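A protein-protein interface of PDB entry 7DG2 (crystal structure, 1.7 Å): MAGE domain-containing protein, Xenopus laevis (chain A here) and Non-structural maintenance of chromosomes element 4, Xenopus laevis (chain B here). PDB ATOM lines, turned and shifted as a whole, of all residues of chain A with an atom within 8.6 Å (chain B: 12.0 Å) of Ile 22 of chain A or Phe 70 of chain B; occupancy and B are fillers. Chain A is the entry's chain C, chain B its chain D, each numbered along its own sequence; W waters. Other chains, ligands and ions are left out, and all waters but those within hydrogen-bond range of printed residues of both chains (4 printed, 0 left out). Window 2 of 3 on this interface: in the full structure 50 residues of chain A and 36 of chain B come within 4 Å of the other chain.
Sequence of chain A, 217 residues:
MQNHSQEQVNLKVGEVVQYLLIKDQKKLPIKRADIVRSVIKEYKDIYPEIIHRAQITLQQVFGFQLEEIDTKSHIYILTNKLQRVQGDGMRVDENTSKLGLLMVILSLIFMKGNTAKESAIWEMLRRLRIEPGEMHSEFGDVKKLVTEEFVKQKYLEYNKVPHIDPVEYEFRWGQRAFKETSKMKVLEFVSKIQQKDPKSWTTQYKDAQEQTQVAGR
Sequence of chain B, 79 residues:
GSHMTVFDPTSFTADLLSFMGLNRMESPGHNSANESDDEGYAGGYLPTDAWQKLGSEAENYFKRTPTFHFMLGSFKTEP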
ATOM      1  N   GLY A  14      -9.231 -20.603 -25.749  1.00  0.00           N
ATOM      2  CA  GLY A  14      -8.373 -19.540 -25.246  1.00  0.00           C
ATOM      3  C   GLY A  14      -8.976 -18.815 -24.057  1.00  0.00           C
ATOM      4  O   GLY A  14      -8.271 -18.474 -23.102  1.00  0.00           O
ATOM      5  N   GLU A  15     -10.287 -18.572 -24.097  1.00  0.00           N
ATOM      6  CA  GLU A  15     -10.944 -17.908 -22.975  1.00  0.00           C
ATOM      7  C   GLU A  15     -10.883 -18.759 -21.714  1.00  0.00           C
ATOM      8  O   GLU A  15     -10.718 -18.236 -20.606  1.00  0.00           O
ATOM      9  CB  GLU A  15     -12.395 -17.578 -23.349  1.00  0.00           C
ATOM     10  CG  GLU A  15     -12.463 -16.529 -24.443  1.00  0.00           C
ATOM     11  CD  GLU A  15     -13.822 -16.409 -25.124  1.00  0.00           C
ATOM     12  OE1 GLU A  15     -14.752 -17.167 -24.794  1.00  0.00           O
ATOM     13  OE2 GLU A  15     -13.948 -15.545 -26.020  1.00  0.00           O
ATOM     14  N   VAL A  16     -11.052 -20.075 -21.852  1.00  0.00           N
ATOM     15  CA  VAL A  16     -10.970 -20.940 -20.678  1.00  0.00           C
ATOM     16  C   VAL A  16      -9.565 -20.904 -20.085  1.00  0.00           C
ATOM     17  O   VAL A  16      -9.394 -20.900 -18.859  1.00  0.00           O
ATOM     18  CB  VAL A  16     -11.393 -22.376 -21.037  1.00  0.00           C
ATOM     19  CG1 VAL A  16     -11.064 -23.306 -19.891  1.00  0.00           C
ATOM     20  CG2 VAL A  16     -12.905 -22.406 -21.344  1.00  0.00           C
ATOM     21  N   VAL A  17      -8.534 -20.921 -20.940  1.00  0.00           N
ATOM     22  CA  VAL A  17      -7.162 -20.822 -20.438  1.00  0.00           C
ATOM     23  C   VAL A  17      -6.979 -19.516 -19.678  1.00  0.00           C
ATOM     24  O   VAL A  17      -6.431 -19.493 -18.574  1.00  0.00           O
ATOM     25  CB  VAL A  17      -6.146 -20.951 -21.588  1.00  0.00           C
ATOM     26  CG1 VAL A  17      -4.716 -20.682 -21.089  1.00  0.00           C
ATOM     27  CG2 VAL A  17      -6.246 -22.331 -22.226  1.00  0.00           C
ATOM     28  N   GLN A  18      -7.453 -18.411 -20.257  1.00  0.00           N
ATOM     29  CA  GLN A  18      -7.339 -17.125 -19.565  1.00  0.00           C
ATOM     30  C   GLN A  18      -8.038 -17.172 -18.217  1.00  0.00           C
ATOM     31  O   GLN A  18      -7.514 -16.672 -17.215  1.00  0.00           O
ATOM     32  CB  GLN A  18      -7.947 -16.004 -20.402  1.00  0.00           C
ATOM     33  CG  GLN A  18      -7.214 -15.658 -21.661  1.00  0.00           C
ATOM     34  CD  GLN A  18      -7.881 -14.491 -22.354  1.00  0.00           C
ATOM     35  OE1 GLN A  18      -8.674 -14.681 -23.284  1.00  0.00           O
ATOM     36  NE2 GLN A  18      -7.591 -13.269 -21.884  1.00  0.00           N
ATOM     37  N   TYR A  19      -9.240 -17.751 -18.188  1.00  0.00           N
ATOM     38  CA  TYR A  19     -10.009 -17.827 -16.955  1.00  0.00           C
ATOM     39  C   TYR A  19      -9.278 -18.656 -15.910  1.00  0.00           C
ATOM     40  O   TYR A  19      -9.215 -18.273 -14.736  1.00  0.00           O
ATOM     41  CB  TYR A  19     -11.379 -18.432 -17.281  1.00  0.00           C
ATOM     42  CG  TYR A  19     -12.344 -18.565 -16.142  1.00  0.00           C
ATOM     43  CD1 TYR A  19     -13.156 -17.503 -15.774  1.00  0.00           C
ATOM     44  CD2 TYR A  19     -12.495 -19.769 -15.473  1.00  0.00           C
ATOM     45  CE1 TYR A  19     -14.077 -17.639 -14.764  1.00  0.00           C
ATOM     46  CE2 TYR A  19     -13.404 -19.903 -14.452  1.00  0.00           C
ATOM     47  CZ  TYR A  19     -14.189 -18.839 -14.100  1.00  0.00           C
ATOM     48  OH  TYR A  19     -15.109 -18.959 -13.079  1.00  0.00           O
ATOM     49  N   LEU A  20      -8.706 -19.796 -16.318  1.00  0.00           N
ATOM     50  CA  LEU A  20      -7.980 -20.628 -15.358  1.00  0.00           C
ATOM     51  C   LEU A  20      -6.797 -19.877 -14.745  1.00  0.00           C
ATOM     52  O   LEU A  20      -6.568 -19.936 -13.527  1.00  0.00           O
ATOM     53  CB  LEU A  20      -7.514 -21.912 -16.049  1.00  0.00           C
ATOM     54  CG  LEU A  20      -8.682 -22.873 -16.286  1.00  0.00           C
ATOM     55  CD1 LEU A  20      -8.260 -23.965 -17.249  1.00  0.00           C
ATOM     56  CD2 LEU A  20      -9.137 -23.484 -14.956  1.00  0.00           C
ATOM     57  N   LEU A  21      -6.026 -19.171 -15.573  1.00  0.00           N
ATOM     58  CA  LEU A  21      -4.904 -18.396 -15.048  1.00  0.00           C
ATOM     59  C   LEU A  21      -5.380 -17.315 -14.086  1.00  0.00           C
ATOM     60  O   LEU A  21      -4.836 -17.156 -12.983  1.00  0.00           O
ATOM     61  CB  LEU A  21      -4.127 -17.768 -16.205  1.00  0.00           C
ATOM     62  CG  LEU A  21      -3.429 -18.761 -17.119  1.00  0.00           C
ATOM     63  CD1 LEU A  21      -2.840 -17.999 -18.320  1.00  0.00           C
ATOM     64  CD2 LEU A  21      -2.324 -19.484 -16.346  1.00  0.00           C
ATOM     65  N   ILE A  22      -6.421 -16.580 -14.476  1.00  0.00           N
ATOM     66  CA  ILE A  22      -6.850 -15.447 -13.665  1.00  0.00           C
ATOM     67  C   ILE A  22      -7.486 -15.925 -12.368  1.00  0.00           C
ATOM     68  O   ILE A  22      -7.242 -15.359 -11.292  1.00  0.00           O
ATOM     69  CB  ILE A  22      -7.785 -14.546 -14.489  1.00  0.00           C
ATOM     70  CG1 ILE A  22      -6.934 -13.856 -15.569  1.00  0.00           C
ATOM     71  CG2 ILE A  22      -8.520 -13.571 -13.559  1.00  0.00           C
ATOM     72  CD1 ILE A  22      -7.714 -13.238 -16.709  1.00  0.00           C
ATOM     73  N   LYS A  23      -8.271 -17.006 -12.427  1.00  0.00           N
ATOM     74  CA  LYS A  23      -8.859 -17.550 -11.208  1.00  0.00           C
ATOM     75  C   LYS A  23      -7.854 -18.292 -10.330  1.00  0.00           C
ATOM     76  O   LYS A  23      -8.217 -18.675  -9.215  1.00  0.00           O
ATOM     77  CB  LYS A  23     -10.037 -18.472 -11.558  1.00  0.00           C
ATOM     78  CG  LYS A  23     -11.223 -17.691 -12.145  1.00  0.00           C
ATOM     79  CD  LYS A  23     -11.769 -16.668 -11.120  1.00  0.00           C
ATOM     80  CE  LYS A  23     -13.083 -16.051 -11.571  1.00  0.00           C
ATOM     81  NZ  LYS A  23     -13.624 -15.122 -10.522  1.00  0.00           N
ATOM     82  N   ASP A  24      -6.612 -18.495 -10.783  1.00  0.00           N
ATOM     83  CA  ASP A  24      -5.586 -19.077  -9.932  1.00  0.00           C
ATOM     84  C   ASP A  24      -4.816 -18.024  -9.147  1.00  0.00           C
ATOM     85  O   ASP A  24      -3.961 -18.391  -8.333  1.00  0.00           O
ATOM     86  CB  ASP A  24      -4.589 -19.909 -10.777  1.00  0.00           C
ATOM     87  CG  ASP A  24      -3.702 -20.829  -9.927  1.00  0.00           C
ATOM     88  OD1 ASP A  24      -4.245 -21.544  -9.057  1.00  0.00           O
ATOM     89  OD2 ASP A  24      -2.467 -20.880 -10.165  1.00  0.00           O
ATOM     90  N   GLN A  25      -5.100 -16.732  -9.370  1.00  0.00           N
ATOM     91  CA  GLN A  25      -4.205 -15.686  -8.871  1.00  0.00           C
ATOM     92  C   GLN A  25      -4.014 -15.740  -7.361  1.00  0.00           C
ATOM     93  O   GLN A  25      -2.936 -15.382  -6.870  1.00  0.00           O
ATOM     94  CB  GLN A  25      -4.705 -14.299  -9.274  1.00  0.00           C
ATOM     95  CG  GLN A  25      -4.407 -13.933 -10.729  1.00  0.00           C
ATOM     96  CD  GLN A  25      -4.947 -12.566 -11.095  1.00  0.00           C
ATOM     97  OE1 GLN A  25      -5.879 -12.070 -10.460  1.00  0.00           O
ATOM     98  NE2 GLN A  25      -4.371 -11.952 -12.125  1.00  0.00           N
ATOM     99  N   LYS A  26      -5.043 -16.127  -6.604  1.00  0.00           N
ATOM    100  CA  LYS A  26      -4.922 -16.221  -5.150  1.00  0.00           C
ATOM    101  C   LYS A  26      -5.042 -17.655  -4.652  1.00  0.00           C
ATOM    102  O   LYS A  26      -5.319 -17.879  -3.465  1.00  0.00           O
ATOM    103  CB  LYS A  26      -5.951 -15.317  -4.468  1.00  0.00           C
ATOM    104  CG  LYS A  26      -5.695 -13.834  -4.758  1.00  0.00           C
ATOM    105  CD  LYS A  26      -6.506 -12.923  -3.851  1.00  0.00           C
ATOM    106  CE  LYS A  26      -6.259 -11.457  -4.194  1.00  0.00           C
ATOM    107  NZ  LYS A  26      -4.848 -11.053  -3.995  1.00  0.00           N
ATOM    108  N   LYS A  27      -4.810 -18.627  -5.544  1.00  0.00           N
ATOM    109  CA  LYS A  27      -4.809 -20.054  -5.215  1.00  0.00           C
ATOM    110  C   LYS A  27      -6.132 -20.498  -4.596  1.00  0.00           C
ATOM    111  O   LYS A  27      -6.175 -21.432  -3.790  1.00  0.00           O
ATOM    112  CB  LYS A  27      -3.631 -20.424  -4.306  1.00  0.00           C
ATOM    113  CG  LYS A  27      -2.261 -20.166  -4.947  1.00  0.00           C
ATOM    114  CD  LYS A  27      -2.098 -20.957  -6.232  1.00  0.00           C
ATOM    115  CE  LYS A  27      -0.766 -20.617  -6.920  1.00  0.00           C
ATOM    116  NZ  LYS A  27      -0.544 -21.439  -8.149  1.00  0.00           N
ATOM    117  N   LEU A  28      -7.225 -19.835  -4.972  1.00  0.00           N
ATOM    118  CA  LEU A  28      -8.535 -20.401  -4.676  1.00  0.00           C
ATOM    119  C   LEU A  28      -8.882 -21.456  -5.726  1.00  0.00           C
ATOM    120  O   LEU A  28      -8.664 -21.237  -6.921  1.00  0.00           O
ATOM    121  CB  LEU A  28      -9.604 -19.306  -4.658  1.00  0.00           C
ATOM    122  CG  LEU A  28      -9.374 -18.194  -3.639  1.00  0.00           C
ATOM    123  CD1 LEU A  28     -10.506 -17.163  -3.687  1.00  0.00           C
ATOM    124  CD2 LEU A  28      -9.221 -18.791  -2.245  1.00  0.00           C
ATOM    125  N   ILE A  30     -10.890 -23.812  -8.431  1.00  0.00           N
ATOM    126  CA  ILE A  30     -11.715 -23.372  -9.550  1.00  0.00           C
ATOM    127  C   ILE A  30     -12.760 -24.450  -9.825  1.00  0.00           C
ATOM    128  O   ILE A  30     -12.409 -25.569 -10.213  1.00  0.00           O
ATOM    129  CB  ILE A  30     -10.864 -23.108 -10.799  1.00  0.00           C
ATOM    130  CG1 ILE A  30      -9.691 -22.189 -10.428  1.00  0.00           C
ATOM    131  CG2 ILE A  30     -11.749 -22.541 -11.915  1.00  0.00           C
ATOM    132  CD1 ILE A  30      -8.551 -22.149 -11.465  1.00  0.00           C
ATOM    133  N   LEU A  58      -2.358 -25.552 -21.318  1.00  0.00           N
ATOM    134  CA  LEU A  58      -1.642 -25.224 -20.088  1.00  0.00           C
ATOM    135  C   LEU A  58      -0.445 -26.150 -19.877  1.00  0.00           C
ATOM    136  O   LEU A  58       0.622 -25.703 -19.436  1.00  0.00           O
ATOM    137  CB  LEU A  58      -2.602 -25.284 -18.899  1.00  0.00           C
ATOM    138  CG  LEU A  58      -3.541 -24.080 -18.804  1.00  0.00           C
ATOM    139  CD1 LEU A  58      -4.715 -24.429 -17.909  1.00  0.00           C
ATOM    140  CD2 LEU A  58      -2.784 -22.895 -18.256  1.00  0.00           C
ATOM    141  N   LEU A  78      -4.188 -25.768 -10.313  1.00  0.00           N
ATOM    142  CA  LEU A  78      -3.081 -25.877 -11.254  1.00  0.00           C
ATOM    143  C   LEU A  78      -1.821 -26.215 -10.468  1.00  0.00           C
ATOM    144  O   LEU A  78      -1.485 -25.511  -9.516  1.00  0.00           O
ATOM    145  CB  LEU A  78      -2.886 -24.561 -12.026  1.00  0.00           C
ATOM    146  CG  LEU A  78      -4.033 -24.104 -12.925  1.00  0.00           C
ATOM    147  CD1 LEU A  78      -3.710 -22.722 -13.495  1.00  0.00           C
ATOM    148  CD2 LEU A  78      -4.277 -25.108 -14.048  1.00  0.00           C
ATOM    149  N   THR B  65       2.583 -23.431  -8.982  1.00  0.00           N
ATOM    150  CA  THR B  65       2.731 -22.667 -10.215  1.00  0.00           C
ATOM    151  C   THR B  65       2.809 -21.181  -9.917  1.00  0.00           C
ATOM    152  O   THR B  65       2.148 -20.695  -8.987  1.00  0.00           O
ATOM    153  CB  THR B  65       1.563 -22.913 -11.170  1.00  0.00           C
ATOM    154  OG1 THR B  65       0.333 -22.599 -10.507  1.00  0.00           O
ATOM    155  CG2 THR B  65       1.533 -24.370 -11.603  1.00  0.00           C
ATOM    156  N   PRO B  66       3.608 -20.444 -10.679  1.00  0.00           N
ATOM    157  CA  PRO B  66       3.503 -18.984 -10.650  1.00  0.00           C
ATOM    158  C   PRO B  66       2.164 -18.565 -11.217  1.00  0.00           C
ATOM    159  O   PRO B  66       1.467 -19.345 -11.876  1.00  0.00           O
ATOM    160  CB  PRO B  66       4.654 -18.521 -11.549  1.00  0.00           C
ATOM    161  CG  PRO B  66       4.794 -19.642 -12.539  1.00  0.00           C
ATOM    162  CD  PRO B  66       4.532 -20.909 -11.733  1.00  0.00           C
ATOM    163  N   THR B  67       1.796 -17.314 -10.938  1.00  0.00           N
ATOM    164  CA  THR B  67       0.508 -16.780 -11.359  1.00  0.00           C
ATOM    165  C   THR B  67       0.725 -15.591 -12.290  1.00  0.00           C
ATOM    166  O   THR B  67       1.763 -14.915 -12.239  1.00  0.00           O
ATOM    167  CB  THR B  67      -0.363 -16.371 -10.142  1.00  0.00           C
ATOM    168  OG1 THR B  67       0.396 -15.542  -9.244  1.00  0.00           O
ATOM    169  CG2 THR B  67      -0.851 -17.615  -9.387  1.00  0.00           C
ATOM    170  N   PHE B  68      -0.260 -15.355 -13.153  1.00  0.00           N
ATOM    171  CA  PHE B  68      -0.200 -14.327 -14.187  1.00  0.00           C
ATOM    172  C   PHE B  68      -0.903 -13.071 -13.698  1.00  0.00           C
ATOM    173  O   PHE B  68      -2.070 -13.130 -13.305  1.00  0.00           O
ATOM    174  CB  PHE B  68      -0.860 -14.835 -15.468  1.00  0.00           C
ATOM    175  CG  PHE B  68      -0.933 -13.813 -16.580  1.00  0.00           C
ATOM    176  CD1 PHE B  68       0.165 -13.032 -16.917  1.00  0.00           C
ATOM    177  CD2 PHE B  68      -2.091 -13.685 -17.321  1.00  0.00           C
ATOM    178  CE1 PHE B  68       0.090 -12.111 -17.964  1.00  0.00           C
ATOM    179  CE2 PHE B  68      -2.170 -12.775 -18.382  1.00  0.00           C
ATOM    180  CZ  PHE B  68      -1.086 -11.996 -18.697  1.00  0.00           C
ATOM    181  N   HIS B  69      -0.190 -11.947 -13.730  1.00  0.00           N
ATOM    182  CA  HIS B  69      -0.708 -10.671 -13.255  1.00  0.00           C
ATOM    183  C   HIS B  69      -0.481  -9.607 -14.314  1.00  0.00           C
ATOM    184  O   HIS B  69       0.495  -9.654 -15.062  1.00  0.00           O
ATOM    185  CB  HIS B  69      -0.040 -10.273 -11.938  1.00  0.00           C
ATOM    186  CG  HIS B  69      -0.290 -11.266 -10.847  1.00  0.00           C
ATOM    187  ND1 HIS B  69      -1.335 -11.149  -9.955  1.00  0.00           N
ATOM    188  CD2 HIS B  69       0.339 -12.427 -10.545  1.00  0.00           C
ATOM    189  CE1 HIS B  69      -1.324 -12.186  -9.133  1.00  0.00           C
ATOM    190  NE2 HIS B  69      -0.320 -12.976  -9.471  1.00  0.00           N
ATOM    191  N   PHE B  70      -1.408  -8.652 -14.379  1.00  0.00           N
ATOM    192  CA  PHE B  70      -1.392  -7.642 -15.427  1.00  0.00           C
ATOM    193  C   PHE B  70      -2.217  -6.464 -14.924  1.00  0.00           C
ATOM    194  O   PHE B  70      -2.957  -6.573 -13.941  1.00  0.00           O
ATOM    195  CB  PHE B  70      -1.969  -8.202 -16.733  1.00  0.00           C
ATOM    196  CG  PHE B  70      -3.301  -8.865 -16.527  1.00  0.00           C
ATOM    197  CD1 PHE B  70      -4.469  -8.117 -16.517  1.00  0.00           C
ATOM    198  CD2 PHE B  70      -3.373 -10.217 -16.245  1.00  0.00           C
ATOM    199  CE1 PHE B  70      -5.698  -8.717 -16.271  1.00  0.00           C
ATOM    200  CE2 PHE B  70      -4.600 -10.827 -16.007  1.00  0.00           C
ATOM    201  CZ  PHE B  70      -5.761 -10.071 -16.009  1.00  0.00           C
ATOM    202  N   MET B  71      -2.103  -5.343 -15.627  1.00  0.00           N
ATOM    203  CA  MET B  71      -2.908  -4.159 -15.345  1.00  0.00           C
ATOM    204  C   MET B  71      -3.909  -3.864 -16.454  1.00  0.00           C
ATOM    205  O   MET B  71      -5.088  -3.630 -16.177  1.00  0.00           O
ATOM    206  CB  MET B  71      -1.974  -2.951 -15.129  1.00  0.00           C
ATOM    207  CG  MET B  71      -2.677  -1.665 -14.726  1.00  0.00           C
ATOM    208  SD  MET B  71      -3.532  -1.823 -13.148  1.00  0.00           S
ATOM    209  CE  MET B  71      -2.198  -1.870 -11.947  1.00  0.00           C
ATOM    210  N   LEU B  72      -3.468  -3.877 -17.711  1.00  0.00           N
ATOM    211  CA  LEU B  72      -4.366  -3.651 -18.838  1.00  0.00           C
ATOM    212  C   LEU B  72      -5.535  -4.629 -18.794  1.00  0.00           C
ATOM    213  O   LEU B  72      -5.339  -5.838 -18.635  1.00  0.00           O
ATOM    214  CB  LEU B  72      -3.603  -3.817 -20.154  1.00  0.00           C
ATOM    215  CG  LEU B  72      -4.468  -3.753 -21.418  1.00  0.00           C
ATOM    216  CD1 LEU B  72      -4.914  -2.319 -21.655  1.00  0.00           C
ATOM    217  CD2 LEU B  72      -3.721  -4.292 -22.638  1.00  0.00           C
ATOM    218  N   GLY B  73      -6.759  -4.106 -18.931  1.00  0.00           N
ATOM    219  CA  GLY B  73      -7.925  -4.972 -18.925  1.00  0.00           C
ATOM    220  C   GLY B  73      -8.437  -5.350 -17.553  1.00  0.00           C
ATOM    221  O   GLY B  73      -9.468  -6.033 -17.457  1.00  0.00           O
ATOM    222  N   SER B  74      -7.769  -4.924 -16.487  1.00  0.00           N
ATOM    223  CA  SER B  74      -8.243  -5.234 -15.149  1.00  0.00           C
ATOM    224  C   SER B  74      -9.249  -4.214 -14.631  1.00  0.00           C
ATOM    225  O   SER B  74      -9.883  -4.469 -13.604  1.00  0.00           O
ATOM    226  CB  SER B  74      -7.069  -5.325 -14.171  1.00  0.00           C
ATOM    227  OG  SER B  74      -6.521  -4.036 -13.883  1.00  0.00           O
ATOM    228  N   PHE B  75      -9.411  -3.088 -15.330  1.00  0.00           N
ATOM    229  CA  PHE B  75     -10.240  -1.977 -14.861  1.00  0.00           C
ATOM    230  C   PHE B  75     -11.710  -2.261 -15.125  1.00  0.00           C
ATOM    231  O   PHE B  75     -12.080  -2.652 -16.237  1.00  0.00           O
ATOM    232  CB  PHE B  75      -9.875  -0.675 -15.580  1.00  0.00           C
ATOM    233  CG  PHE B  75      -8.430  -0.293 -15.497  1.00  0.00           C
ATOM    234  CD1 PHE B  75      -7.680  -0.568 -14.375  1.00  0.00           C
ATOM    235  CD2 PHE B  75      -7.827   0.374 -16.559  1.00  0.00           C
ATOM    236  CE1 PHE B  75      -6.342  -0.188 -14.308  1.00  0.00           C
ATOM    237  CE2 PHE B  75      -6.498   0.744 -16.503  1.00  0.00           C
ATOM    238  CZ  PHE B  75      -5.754   0.463 -15.371  1.00  0.00           C
ATOM    239  N   LYS B  76     -12.555  -2.013 -14.126  1.00  0.00           N
ATOM    240  CA  LYS B  76     -14.008  -2.132 -14.282  1.00  0.00           C
ATOM    241  C   LYS B  76     -14.616  -0.734 -14.171  1.00  0.00           C
ATOM    242  O   LYS B  76     -14.948  -0.276 -13.077  1.00  0.00           O
ATOM    243  CB  LYS B  76     -14.610  -3.084 -13.236  1.00  0.00           C
ATOM    244  CG  LYS B  76     -16.137  -3.208 -13.325  1.00  0.00           C
ATOM    245  CD  LYS B  76     -16.792  -3.257 -11.943  1.00  0.00           C
ATOM    246  CE  LYS B  76     -17.980  -2.295 -11.857  1.00  0.00           C
ATOM    247  NZ  LYS B  76     -18.625  -2.277 -10.507  1.00  0.00           N
ATOM    248  N   THR B  77     -14.763  -0.053 -15.307  1.00  0.00           N
ATOM    249  CA  THR B  77     -14.321  -0.540 -16.608  1.00  0.00           C
ATOM    250  C   THR B  77     -13.387   0.486 -17.247  1.00  0.00           C
ATOM    251  O   THR B  77     -13.036   1.483 -16.619  1.00  0.00           O
ATOM    252  CB  THR B  77     -15.506  -0.820 -17.553  1.00  0.00           C
ATOM    253  OG1 THR B  77     -16.275   0.377 -17.729  1.00  0.00           O
ATOM    254  CG2 THR B  77     -16.403  -1.915 -16.981  1.00  0.00           C
HETATM  255  O   HOH W   1      -1.157 -20.119 -12.400  1.00  0.00           O
HETATM  256  O   HOH W   2      -0.056 -24.180  -7.602  1.00  0.00           O
HETATM  257  O   HOH W   3      -3.787  -9.004 -12.532  1.00  0.00           O
HETATM  258  O   HOH W   4      -2.179 -17.528 -13.039  1.00  0.00           O
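OD2 of Asp 24 of chain A lies within salt-bridge range of NZ of Lys 27 of chain A (2.8 Å).
The side-chain hydroxyl (OG1) of Thr 67 of chain B lies within hydrogen-bond range of a ring nitrogen (NE2) of His 69 of chain B.
No residue of chain B comes within 4 Å of Leu 21 of chain A.
Ile 22 of chain A touches just one residue of chain B: Phe 70.
No residue of chain B comes within 4 Å of Lys 23 of chain A.
Asp 24 of chain A touches just these residues of chain B: Thr 65 and Thr 67.
Gln 25 of chain A touches just these residues of chain B: Thr 67, Phe 68 and His 69.
Of the printed residues of chain A, Thr 67 of chain B touches Asp 24 (3.4 Å), Gln 25 (3.9 Å) and Lys 27 (3.9 Å).
Printed residues of chain A within 4 Å of Phe 68 of chain B: Gln 25.
Printed residues of chain A within 4 Å of His 69 of chain B: Gln 25 (3.8 Å).
Phe 70 of chain B touches just one residue of chain A: Ile 22 (3.8 Å).
The nearest printed residue of chain A that does not touch Phe 68 of chain B is Leu 21 of chain A (4.5 Å).
Water W4 bridges O of Leu 21 of chain A (2.7 Å) and N of Phe 68 of chain B (2.9 Å).
Water W1 lies within hydrogen-bond range of the side-chain carboxylate of Asp 24 of chain A (2.7 Å), the backbone carbonyl oxygen of Pro 66 of chain B (2.8 Å) and the side-chain hydroxyl of Thr 65 of chain B (3.5 Å).
Water W2 lies within hydrogen-bond range of the backbone carbonyl oxygen (O) of Leu 78 of chain A, the side-chain amino group (NZ) of Lys 27 of chain A and the backbone NH (N) of Thr 65 of chain B.
Water W3 bridges the backbone carbonyl oxygen of Phe 70 of chain B and the side-chain amide nitrogen of Gln 25 of chain A.
The side-chain carboxylate (OD2) of Asp 24 of chain A sits at hydrogen-bond distance from the side-chain hydroxyl (OG1) of Thr 65 of chain B, 3.3 Å away.
NE2 of Gln 25 of chain A lies within hydrogen-bond range of O of Phe 68 of chain B (2.8 Å).
The side-chain hydroxyl of Thr 65 of chain B lies within hydrogen-bond range of the side-chain amino group of Lys 27 of chain A (2.8 Å).
Among the printed residues, merely in contact across the chains: Ile 22 of chain A with Phe 70 of chain B (3.8 Å), Asp 24 of chain A with Thr 67 of chain B (3.4 Å), Gln 25 of chain A with Thr 67 of chain B (3.9 Å), Gln 25 of chain A with His 69 of chain B (3.8 Å), Lys 27 of chain A with Thr 67 of chain B (3.9 Å) and Leu 78 of chain A with Thr 65 of chain B (3.6 Å).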
